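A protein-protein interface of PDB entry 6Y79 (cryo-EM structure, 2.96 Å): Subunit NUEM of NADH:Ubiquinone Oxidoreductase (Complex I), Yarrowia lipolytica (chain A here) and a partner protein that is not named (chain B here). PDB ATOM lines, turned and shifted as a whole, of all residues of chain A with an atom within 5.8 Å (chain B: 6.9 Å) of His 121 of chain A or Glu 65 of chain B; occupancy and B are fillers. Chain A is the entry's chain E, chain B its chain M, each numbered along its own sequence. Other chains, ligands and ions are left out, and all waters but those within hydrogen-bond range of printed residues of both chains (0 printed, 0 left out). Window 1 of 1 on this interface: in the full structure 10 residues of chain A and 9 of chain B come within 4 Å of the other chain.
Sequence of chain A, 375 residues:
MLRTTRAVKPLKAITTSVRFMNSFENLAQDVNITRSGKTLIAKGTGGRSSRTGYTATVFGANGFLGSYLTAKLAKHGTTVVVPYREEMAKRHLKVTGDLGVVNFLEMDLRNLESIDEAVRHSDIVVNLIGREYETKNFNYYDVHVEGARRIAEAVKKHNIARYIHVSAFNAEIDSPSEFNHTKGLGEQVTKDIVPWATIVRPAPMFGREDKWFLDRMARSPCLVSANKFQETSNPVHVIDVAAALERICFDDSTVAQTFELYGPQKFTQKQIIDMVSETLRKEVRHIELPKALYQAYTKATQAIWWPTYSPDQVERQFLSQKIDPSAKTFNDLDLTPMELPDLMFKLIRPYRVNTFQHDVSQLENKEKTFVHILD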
ATOM      1  N   THR A  55      -4.290  10.336 -32.197  1.00  0.00           N
ATOM      2  CA  THR A  55      -3.398  11.485 -32.209  1.00  0.00           C
ATOM      3  C   THR A  55      -2.929  11.704 -33.644  1.00  0.00           C
ATOM      4  O   THR A  55      -2.426  10.776 -34.299  1.00  0.00           O
ATOM      5  CB  THR A  55      -2.226  11.299 -31.245  1.00  0.00           C
ATOM      6  OG1 THR A  55      -2.736  11.103 -29.924  1.00  0.00           O
ATOM      7  CG2 THR A  55      -1.362  12.534 -31.228  1.00  0.00           C
ATOM      8  N   LEU A 105       3.426  23.242 -31.490  1.00  0.00           N
ATOM      9  CA  LEU A 105       4.856  23.150 -31.214  1.00  0.00           C
ATOM     10  C   LEU A 105       5.633  23.651 -32.421  1.00  0.00           C
ATOM     11  O   LEU A 105       5.217  23.456 -33.564  1.00  0.00           O
ATOM     12  CB  LEU A 105       5.277  21.727 -30.825  1.00  0.00           C
ATOM     13  CG  LEU A 105       5.613  20.654 -31.850  1.00  0.00           C
ATOM     14  CD1 LEU A 105       6.235  19.482 -31.127  1.00  0.00           C
ATOM     15  CD2 LEU A 105       4.381  20.222 -32.597  1.00  0.00           C
ATOM     16  N   GLU A 117      10.321  14.650 -33.965  1.00  0.00           N
ATOM     17  CA  GLU A 117       9.702  14.854 -32.656  1.00  0.00           C
ATOM     18  C   GLU A 117       8.220  15.215 -32.738  1.00  0.00           C
ATOM     19  O   GLU A 117       7.445  14.808 -31.862  1.00  0.00           O
ATOM     20  CB  GLU A 117      10.449  15.963 -31.896  1.00  0.00           C
ATOM     21  CG  GLU A 117      10.035  16.242 -30.444  1.00  0.00           C
ATOM     22  CD  GLU A 117      10.864  17.361 -29.809  1.00  0.00           C
ATOM     23  OE1 GLU A 117      11.754  17.884 -30.494  1.00  0.00           O
ATOM     24  OE2 GLU A 117      10.615  17.732 -28.637  1.00  0.00           O
ATOM     25  N   ALA A 118       7.791  15.942 -33.774  1.00  0.00           N
ATOM     26  CA  ALA A 118       6.361  16.218 -33.901  1.00  0.00           C
ATOM     27  C   ALA A 118       5.553  14.981 -34.291  1.00  0.00           C
ATOM     28  O   ALA A 118       4.348  14.928 -34.026  1.00  0.00           O
ATOM     29  CB  ALA A 118       6.111  17.332 -34.915  1.00  0.00           C
ATOM     30  N   VAL A 119       6.182  13.983 -34.906  1.00  0.00           N
ATOM     31  CA  VAL A 119       5.458  12.813 -35.395  1.00  0.00           C
ATOM     32  C   VAL A 119       5.636  11.638 -34.449  1.00  0.00           C
ATOM     33  O   VAL A 119       5.233  10.513 -34.761  1.00  0.00           O
ATOM     34  CB  VAL A 119       5.918  12.425 -36.811  1.00  0.00           C
ATOM     35  CG1 VAL A 119       5.770  13.588 -37.751  1.00  0.00           C
ATOM     36  CG2 VAL A 119       7.346  11.958 -36.786  1.00  0.00           C
ATOM     37  N   ARG A 120       6.227  11.888 -33.284  1.00  0.00           N
ATOM     38  CA  ARG A 120       6.662  10.794 -32.423  1.00  0.00           C
ATOM     39  C   ARG A 120       5.494  10.065 -31.773  1.00  0.00           C
ATOM     40  O   ARG A 120       5.559   8.847 -31.563  1.00  0.00           O
ATOM     41  CB  ARG A 120       7.604  11.341 -31.362  1.00  0.00           C
ATOM     42  CG  ARG A 120       8.299  10.292 -30.557  1.00  0.00           C
ATOM     43  CD  ARG A 120       9.197  10.949 -29.555  1.00  0.00           C
ATOM     44  NE  ARG A 120      10.380  11.516 -30.178  1.00  0.00           N
ATOM     45  CZ  ARG A 120      11.266  12.260 -29.531  1.00  0.00           C
ATOM     46  NH1 ARG A 120      12.327  12.735 -30.166  1.00  0.00           N
ATOM     47  NH2 ARG A 120      11.089  12.525 -28.243  1.00  0.00           N
ATOM     48  N   HIS A 121       4.414  10.781 -31.466  1.00  0.00           N
ATOM     49  CA  HIS A 121       3.255  10.199 -30.800  1.00  0.00           C
ATOM     50  C   HIS A 121       2.014  10.211 -31.669  1.00  0.00           C
ATOM     51  O   HIS A 121       0.943   9.798 -31.205  1.00  0.00           O
ATOM     52  CB  HIS A 121       2.975  10.935 -29.493  1.00  0.00           C
ATOM     53  CG  HIS A 121       4.133  10.930 -28.550  1.00  0.00           C
ATOM     54  ND1 HIS A 121       4.487   9.818 -27.819  1.00  0.00           N
ATOM     55  CD2 HIS A 121       5.035  11.889 -28.243  1.00  0.00           C
ATOM     56  CE1 HIS A 121       5.552  10.097 -27.090  1.00  0.00           C
ATOM     57  NE2 HIS A 121       5.903  11.347 -27.329  1.00  0.00           N
ATOM     58  N   SER A 122       2.126  10.686 -32.906  1.00  0.00           N
ATOM     59  CA  SER A 122       1.029  10.604 -33.854  1.00  0.00           C
ATOM     60  C   SER A 122       0.757   9.146 -34.182  1.00  0.00           C
ATOM     61  O   SER A 122       1.692   8.351 -34.309  1.00  0.00           O
ATOM     62  CB  SER A 122       1.381  11.343 -35.139  1.00  0.00           C
ATOM     63  OG  SER A 122       2.097  12.523 -34.876  1.00  0.00           O
ATOM     64  N   ASP A 123      -0.524   8.771 -34.246  1.00  0.00           N
ATOM     65  CA  ASP A 123      -0.840   7.541 -34.960  1.00  0.00           C
ATOM     66  C   ASP A 123      -1.369   7.800 -36.359  1.00  0.00           C
ATOM     67  O   ASP A 123      -1.410   6.859 -37.151  1.00  0.00           O
ATOM     68  CB  ASP A 123      -1.804   6.625 -34.183  1.00  0.00           C
ATOM     69  CG  ASP A 123      -3.050   7.312 -33.653  1.00  0.00           C
ATOM     70  OD1 ASP A 123      -3.809   7.972 -34.413  1.00  0.00           O
ATOM     71  OD2 ASP A 123      -3.337   7.114 -32.450  1.00  0.00           O
ATOM     72  N   SER B  23       6.155   3.880 -25.884  1.00  0.00           N
ATOM     73  CA  SER B  23       5.121   4.882 -26.178  1.00  0.00           C
ATOM     74  C   SER B  23       3.928   4.296 -26.935  1.00  0.00           C
ATOM     75  O   SER B  23       3.567   4.761 -28.019  1.00  0.00           O
ATOM     76  CB  SER B  23       5.730   6.042 -26.955  1.00  0.00           C
ATOM     77  OG  SER B  23       4.725   6.896 -27.459  1.00  0.00           O
ATOM     78  N   TYR B  24       3.345   3.224 -26.370  1.00  0.00           N
ATOM     79  CA  TYR B  24       2.107   2.565 -26.814  1.00  0.00           C
ATOM     80  C   TYR B  24       2.163   1.985 -28.227  1.00  0.00           C
ATOM     81  O   TYR B  24       1.154   1.479 -28.726  1.00  0.00           O
ATOM     82  CB  TYR B  24       0.899   3.518 -26.728  1.00  0.00           C
ATOM     83  CG  TYR B  24       0.393   3.847 -25.338  1.00  0.00           C
ATOM     84  CD1 TYR B  24       0.738   3.074 -24.240  1.00  0.00           C
ATOM     85  CD2 TYR B  24      -0.451   4.936 -25.134  1.00  0.00           C
ATOM     86  CE1 TYR B  24       0.268   3.384 -22.974  1.00  0.00           C
ATOM     87  CE2 TYR B  24      -0.927   5.253 -23.868  1.00  0.00           C
ATOM     88  CZ  TYR B  24      -0.559   4.466 -22.793  1.00  0.00           C
ATOM     89  OH  TYR B  24      -1.021   4.761 -21.532  1.00  0.00           O
ATOM     90  N   ASN B  25       3.332   2.057 -28.867  1.00  0.00           N
ATOM     91  CA  ASN B  25       3.502   1.775 -30.282  1.00  0.00           C
ATOM     92  C   ASN B  25       4.804   1.055 -30.569  1.00  0.00           C
ATOM     93  O   ASN B  25       5.086   0.777 -31.737  1.00  0.00           O
ATOM     94  CB  ASN B  25       3.504   3.080 -31.102  1.00  0.00           C
ATOM     95  CG  ASN B  25       2.198   3.821 -31.043  1.00  0.00           C
ATOM     96  OD1 ASN B  25       1.128   3.229 -31.140  1.00  0.00           O
ATOM     97  ND2 ASN B  25       2.278   5.138 -30.909  1.00  0.00           N
ATOM     98  N   ASN B  27       7.590   2.703 -29.926  1.00  0.00           N
ATOM     99  CA  ASN B  27       8.492   3.827 -29.713  1.00  0.00           C
ATOM    100  C   ASN B  27       8.902   3.848 -28.249  1.00  0.00           C
ATOM    101  O   ASN B  27       8.053   3.696 -27.372  1.00  0.00           O
ATOM    102  CB  ASN B  27       7.823   5.158 -30.067  1.00  0.00           C
ATOM    103  CG  ASN B  27       7.210   5.170 -31.451  1.00  0.00           C
ATOM    104  OD1 ASN B  27       5.992   5.268 -31.594  1.00  0.00           O
ATOM    105  ND2 ASN B  27       8.048   5.097 -32.478  1.00  0.00           N
ATOM    106  N   ILE B  29      10.530   6.487 -25.659  1.00  0.00           N
ATOM    107  CA  ILE B  29      10.885   7.874 -25.428  1.00  0.00           C
ATOM    108  C   ILE B  29      11.777   7.921 -24.201  1.00  0.00           C
ATOM    109  O   ILE B  29      11.691   7.060 -23.312  1.00  0.00           O
ATOM    110  CB  ILE B  29       9.600   8.707 -25.299  1.00  0.00           C
ATOM    111  CG1 ILE B  29       8.661   7.975 -24.359  1.00  0.00           C
ATOM    112  CG2 ILE B  29       8.946   8.778 -26.638  1.00  0.00           C
ATOM    113  CD1 ILE B  29       7.175   8.396 -24.355  1.00  0.00           C
ATOM    114  N   TYR B  57       4.247   9.882 -17.789  1.00  0.00           N
ATOM    115  CA  TYR B  57       4.969  10.183 -19.010  1.00  0.00           C
ATOM    116  C   TYR B  57       4.615   9.200 -20.132  1.00  0.00           C
ATOM    117  O   TYR B  57       4.567   9.576 -21.281  1.00  0.00           O
ATOM    118  CB  TYR B  57       6.462  10.198 -18.713  1.00  0.00           C
ATOM    119  CG  TYR B  57       6.923  11.401 -17.870  1.00  0.00           C
ATOM    120  CD1 TYR B  57       6.750  12.698 -18.338  1.00  0.00           C
ATOM    121  CD2 TYR B  57       7.579  11.240 -16.648  1.00  0.00           C
ATOM    122  CE1 TYR B  57       7.176  13.778 -17.592  1.00  0.00           C
ATOM    123  CE2 TYR B  57       8.003  12.324 -15.902  1.00  0.00           C
ATOM    124  CZ  TYR B  57       7.802  13.593 -16.381  1.00  0.00           C
ATOM    125  OH  TYR B  57       8.226  14.683 -15.633  1.00  0.00           O
ATOM    126  N   LYS B  58       4.262   7.960 -19.824  1.00  0.00           N
ATOM    127  CA  LYS B  58       3.771   7.016 -20.827  1.00  0.00           C
ATOM    128  C   LYS B  58       2.397   7.435 -21.325  1.00  0.00           C
ATOM    129  O   LYS B  58       2.058   7.185 -22.482  1.00  0.00           O
ATOM    130  CB  LYS B  58       3.721   5.594 -20.221  1.00  0.00           C
ATOM    131  CG  LYS B  58       3.287   4.496 -21.129  1.00  0.00           C
ATOM    132  CD  LYS B  58       3.577   3.164 -20.435  1.00  0.00           C
ATOM    133  CE  LYS B  58       3.042   1.981 -21.214  1.00  0.00           C
ATOM    134  NZ  LYS B  58       3.492   0.711 -20.603  1.00  0.00           N
ATOM    135  N   ASN B  60       0.723  10.813 -21.314  1.00  0.00           N
ATOM    136  CA  ASN B  60       0.635  12.040 -22.122  1.00  0.00           C
ATOM    137  C   ASN B  60       1.985  12.756 -22.260  1.00  0.00           C
ATOM    138  O   ASN B  60       2.223  13.772 -21.615  1.00  0.00           O
ATOM    139  CB  ASN B  60      -0.435  12.974 -21.533  1.00  0.00           C
ATOM    140  CG  ASN B  60      -0.264  13.209 -20.033  1.00  0.00           C
ATOM    141  OD1 ASN B  60       0.654  12.682 -19.415  1.00  0.00           O
ATOM    142  ND2 ASN B  60      -1.130  14.027 -19.460  1.00  0.00           N
ATOM    143  N   MET B  61       2.835  12.299 -23.177  1.00  0.00           N
ATOM    144  CA  MET B  61       4.005  13.104 -23.517  1.00  0.00           C
ATOM    145  C   MET B  61       3.859  13.879 -24.800  1.00  0.00           C
ATOM    146  O   MET B  61       4.814  14.561 -25.196  1.00  0.00           O
ATOM    147  CB  MET B  61       5.272  12.255 -23.575  1.00  0.00           C
ATOM    148  CG  MET B  61       5.955  12.321 -22.242  1.00  0.00           C
ATOM    149  SD  MET B  61       7.429  11.278 -22.068  1.00  0.00           S
ATOM    150  CE  MET B  61       8.607  12.133 -23.128  1.00  0.00           C
ATOM    151  N   VAL B  62       2.676  13.815 -25.418  1.00  0.00           N
ATOM    152  CA  VAL B  62       2.287  14.660 -26.540  1.00  0.00           C
ATOM    153  C   VAL B  62       2.431  16.147 -26.214  1.00  0.00           C
ATOM    154  O   VAL B  62       2.640  16.977 -27.109  1.00  0.00           O
ATOM    155  CB  VAL B  62       0.845  14.278 -26.922  1.00  0.00           C
ATOM    156  CG1 VAL B  62       0.371  14.978 -28.168  1.00  0.00           C
ATOM    157  CG2 VAL B  62       0.727  12.771 -27.114  1.00  0.00           C
ATOM    158  N   ARG B  63       2.378  16.503 -24.933  1.00  0.00           N
ATOM    159  CA  ARG B  63       2.430  17.888 -24.490  1.00  0.00           C
ATOM    160  C   ARG B  63       3.549  18.193 -23.503  1.00  0.00           C
ATOM    161  O   ARG B  63       3.576  19.297 -22.950  1.00  0.00           O
ATOM    162  CB  ARG B  63       1.100  18.246 -23.862  1.00  0.00           C
ATOM    163  CG  ARG B  63       0.739  17.235 -22.839  1.00  0.00           C
ATOM    164  CD  ARG B  63      -0.691  17.407 -22.529  1.00  0.00           C
ATOM    165  NE  ARG B  63      -1.019  16.831 -21.247  1.00  0.00           N
ATOM    166  CZ  ARG B  63      -1.551  17.545 -20.275  1.00  0.00           C
ATOM    167  NH1 ARG B  63      -1.744  18.843 -20.452  1.00  0.00           N
ATOM    168  NH2 ARG B  63      -1.841  16.982 -19.119  1.00  0.00           N
ATOM    169  N   PHE B  64       4.447  17.251 -23.228  1.00  0.00           N
ATOM    170  CA  PHE B  64       5.746  17.621 -22.691  1.00  0.00           C
ATOM    171  C   PHE B  64       6.777  17.820 -23.791  1.00  0.00           C
ATOM    172  O   PHE B  64       7.977  17.833 -23.504  1.00  0.00           O
ATOM    173  CB  PHE B  64       6.292  16.563 -21.738  1.00  0.00           C
ATOM    174  CG  PHE B  64       5.474  16.333 -20.512  1.00  0.00           C
ATOM    175  CD1 PHE B  64       5.516  17.207 -19.442  1.00  0.00           C
ATOM    176  CD2 PHE B  64       4.732  15.179 -20.397  1.00  0.00           C
ATOM    177  CE1 PHE B  64       4.786  16.949 -18.300  1.00  0.00           C
ATOM    178  CE2 PHE B  64       3.997  14.917 -19.258  1.00  0.00           C
ATOM    179  CZ  PHE B  64       4.022  15.800 -18.213  1.00  0.00           C
ATOM    180  N   GLU B  65       6.352  17.921 -25.044  1.00  0.00           N
ATOM    181  CA  GLU B  65       7.305  18.191 -26.103  1.00  0.00           C
ATOM    182  C   GLU B  65       7.601  19.684 -26.139  1.00  0.00           C
ATOM    183  O   GLU B  65       6.745  20.505 -25.790  1.00  0.00           O
ATOM    184  CB  GLU B  65       6.773  17.700 -27.455  1.00  0.00           C
ATOM    185  CG  GLU B  65       6.439  16.201 -27.557  1.00  0.00           C
ATOM    186  CD  GLU B  65       7.616  15.252 -27.270  1.00  0.00           C
ATOM    187  OE1 GLU B  65       8.795  15.663 -27.373  1.00  0.00           O
ATOM    188  OE2 GLU B  65       7.341  14.076 -26.983  1.00  0.00           O
ATOM    189  N   GLN B  66       8.842  20.018 -26.525  1.00  0.00           N
ATOM    190  CA  GLN B  66       9.398  21.381 -26.523  1.00  0.00           C
ATOM    191  C   GLN B  66       9.369  22.020 -25.136  1.00  0.00           C
ATOM    192  O   GLN B  66       9.310  23.245 -25.012  1.00  0.00           O
ATOM    193  CB  GLN B  66       8.693  22.297 -27.530  1.00  0.00           C
ATOM    194  CG  GLN B  66       8.649  21.779 -28.947  1.00  0.00           C
ATOM    195  CD  GLN B  66       9.979  21.879 -29.659  1.00  0.00           C
ATOM    196  OE1 GLN B  66      10.611  20.869 -29.970  1.00  0.00           O
ATOM    197  NE2 GLN B  66      10.412  23.106 -29.924  1.00  0.00           N
ATOM    198  N   LYS B  67       9.421  21.222 -24.075  1.00  0.00           N
ATOM    199  CA  LYS B  67       9.245  21.763 -22.738  1.00  0.00           C
ATOM    200  C   LYS B  67      10.336  21.300 -21.794  1.00  0.00           C
ATOM    201  O   LYS B  67      10.824  20.168 -21.879  1.00  0.00           O
ATOM    202  CB  LYS B  67       7.882  21.402 -22.163  1.00  0.00           C
ATOM    203  CG  LYS B  67       6.811  22.349 -22.627  1.00  0.00           C
ATOM    204  CD  LYS B  67       5.452  21.877 -22.233  1.00  0.00           C
ATOM    205  CE  LYS B  67       4.407  22.489 -23.134  1.00  0.00           C
ATOM    206  NZ  LYS B  67       4.518  23.968 -23.139  1.00  0.00           N
ATOM    207  N   ASP B  68      10.694  22.203 -20.891  1.00  0.00           N
ATOM    208  CA  ASP B  68      11.719  21.943 -19.898  1.00  0.00           C
ATOM    209  C   ASP B  68      11.134  21.155 -18.734  1.00  0.00           C
ATOM    210  O   ASP B  68      10.153  21.580 -18.119  1.00  0.00           O
ATOM    211  CB  ASP B  68      12.281  23.272 -19.403  1.00  0.00           C
ATOM    212  CG  ASP B  68      13.709  23.176 -18.966  1.00  0.00           C
ATOM    213  OD1 ASP B  68      14.305  22.082 -19.087  1.00  0.00           O
ATOM    214  OD2 ASP B  68      14.252  24.203 -18.500  1.00  0.00           O
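Of the printed residues of chain B, Glu 117 of chain A touches Glu 65 (3.0 Å) and Gln 66 (3.2 Å).
His 121 of chain A touches just these residues of chain B: Ser 23, Ile 29, Met 61, Val 62 and Glu 65.
Of the printed residues of chain A, Asn 27 of chain B touches Arg 120.
Printed residues of chain A within 4 Å of Ile 29 of chain B: Arg 120 (3.6 Å) and His 121 (3.6 Å).
Printed residues of chain A within 4 Å of Met 61 of chain B: His 121.
Printed residues of chain A within 4 Å of Gln 66 of chain B: Leu 105 and Glu 117.
The nearest residue of chain B that does not touch His 121 of chain A is Asn 25 of chain B (4.9 Å).
The side-chain amide nitrogen (ND2) of Asn 25 of chain B sits at hydrogen-bond distance from the backbone carbonyl oxygen (O) of Ser 23 of chain B, 3.2 Å away.
The side-chain hydroxyl of Ser 23 of chain B is in hydrogen-bond range of a ring nitrogen (ND1) of His 121 of chain A (3.0 Å).
The guanidinium group (NH2) of Arg 120 of chain A is in salt-bridge range of the side-chain carboxylate (OE1) of Glu 65 of chain B.
The side-chain carboxylate (OE2) of Glu 65 of chain B is in hydrogen-bond range of a ring nitrogen (NE2) of His 121 of chain A (3.1 Å).
The side-chain amide oxygen (OE1) of Gln 66 of chain B lies close to the side-chain carboxylate (OE1) of Glu 117 of chain A, 3.2 Å away.
The side-chain carboxylate of Glu 65 of chain B lies close to the side-chain carboxylate of Glu 117 of chain A (3.0 Å).
CG of Gln 66 of chain B touches CB of Leu 105 of chain A, 3.9 Å away.
Asn 27 of chain B touches Arg 120 of chain A (OD1 to O, 3.6 Å).
Ile 29 of chain B touches Arg 120 of chain A.
CE1 of His 121 of chain A touches CD1 of Ile 29 of chain B, 3.6 Å away.
His 121 of chain A touches Met 61 of chain B.
CB of His 121 of chain A touches CG2 of Val 62 of chain B (3.8 Å).
Of the 16 printed residues of chain B, 7 touch a printed residue of chain A.
Among the printed residues, 11 pairs touch across the chains.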
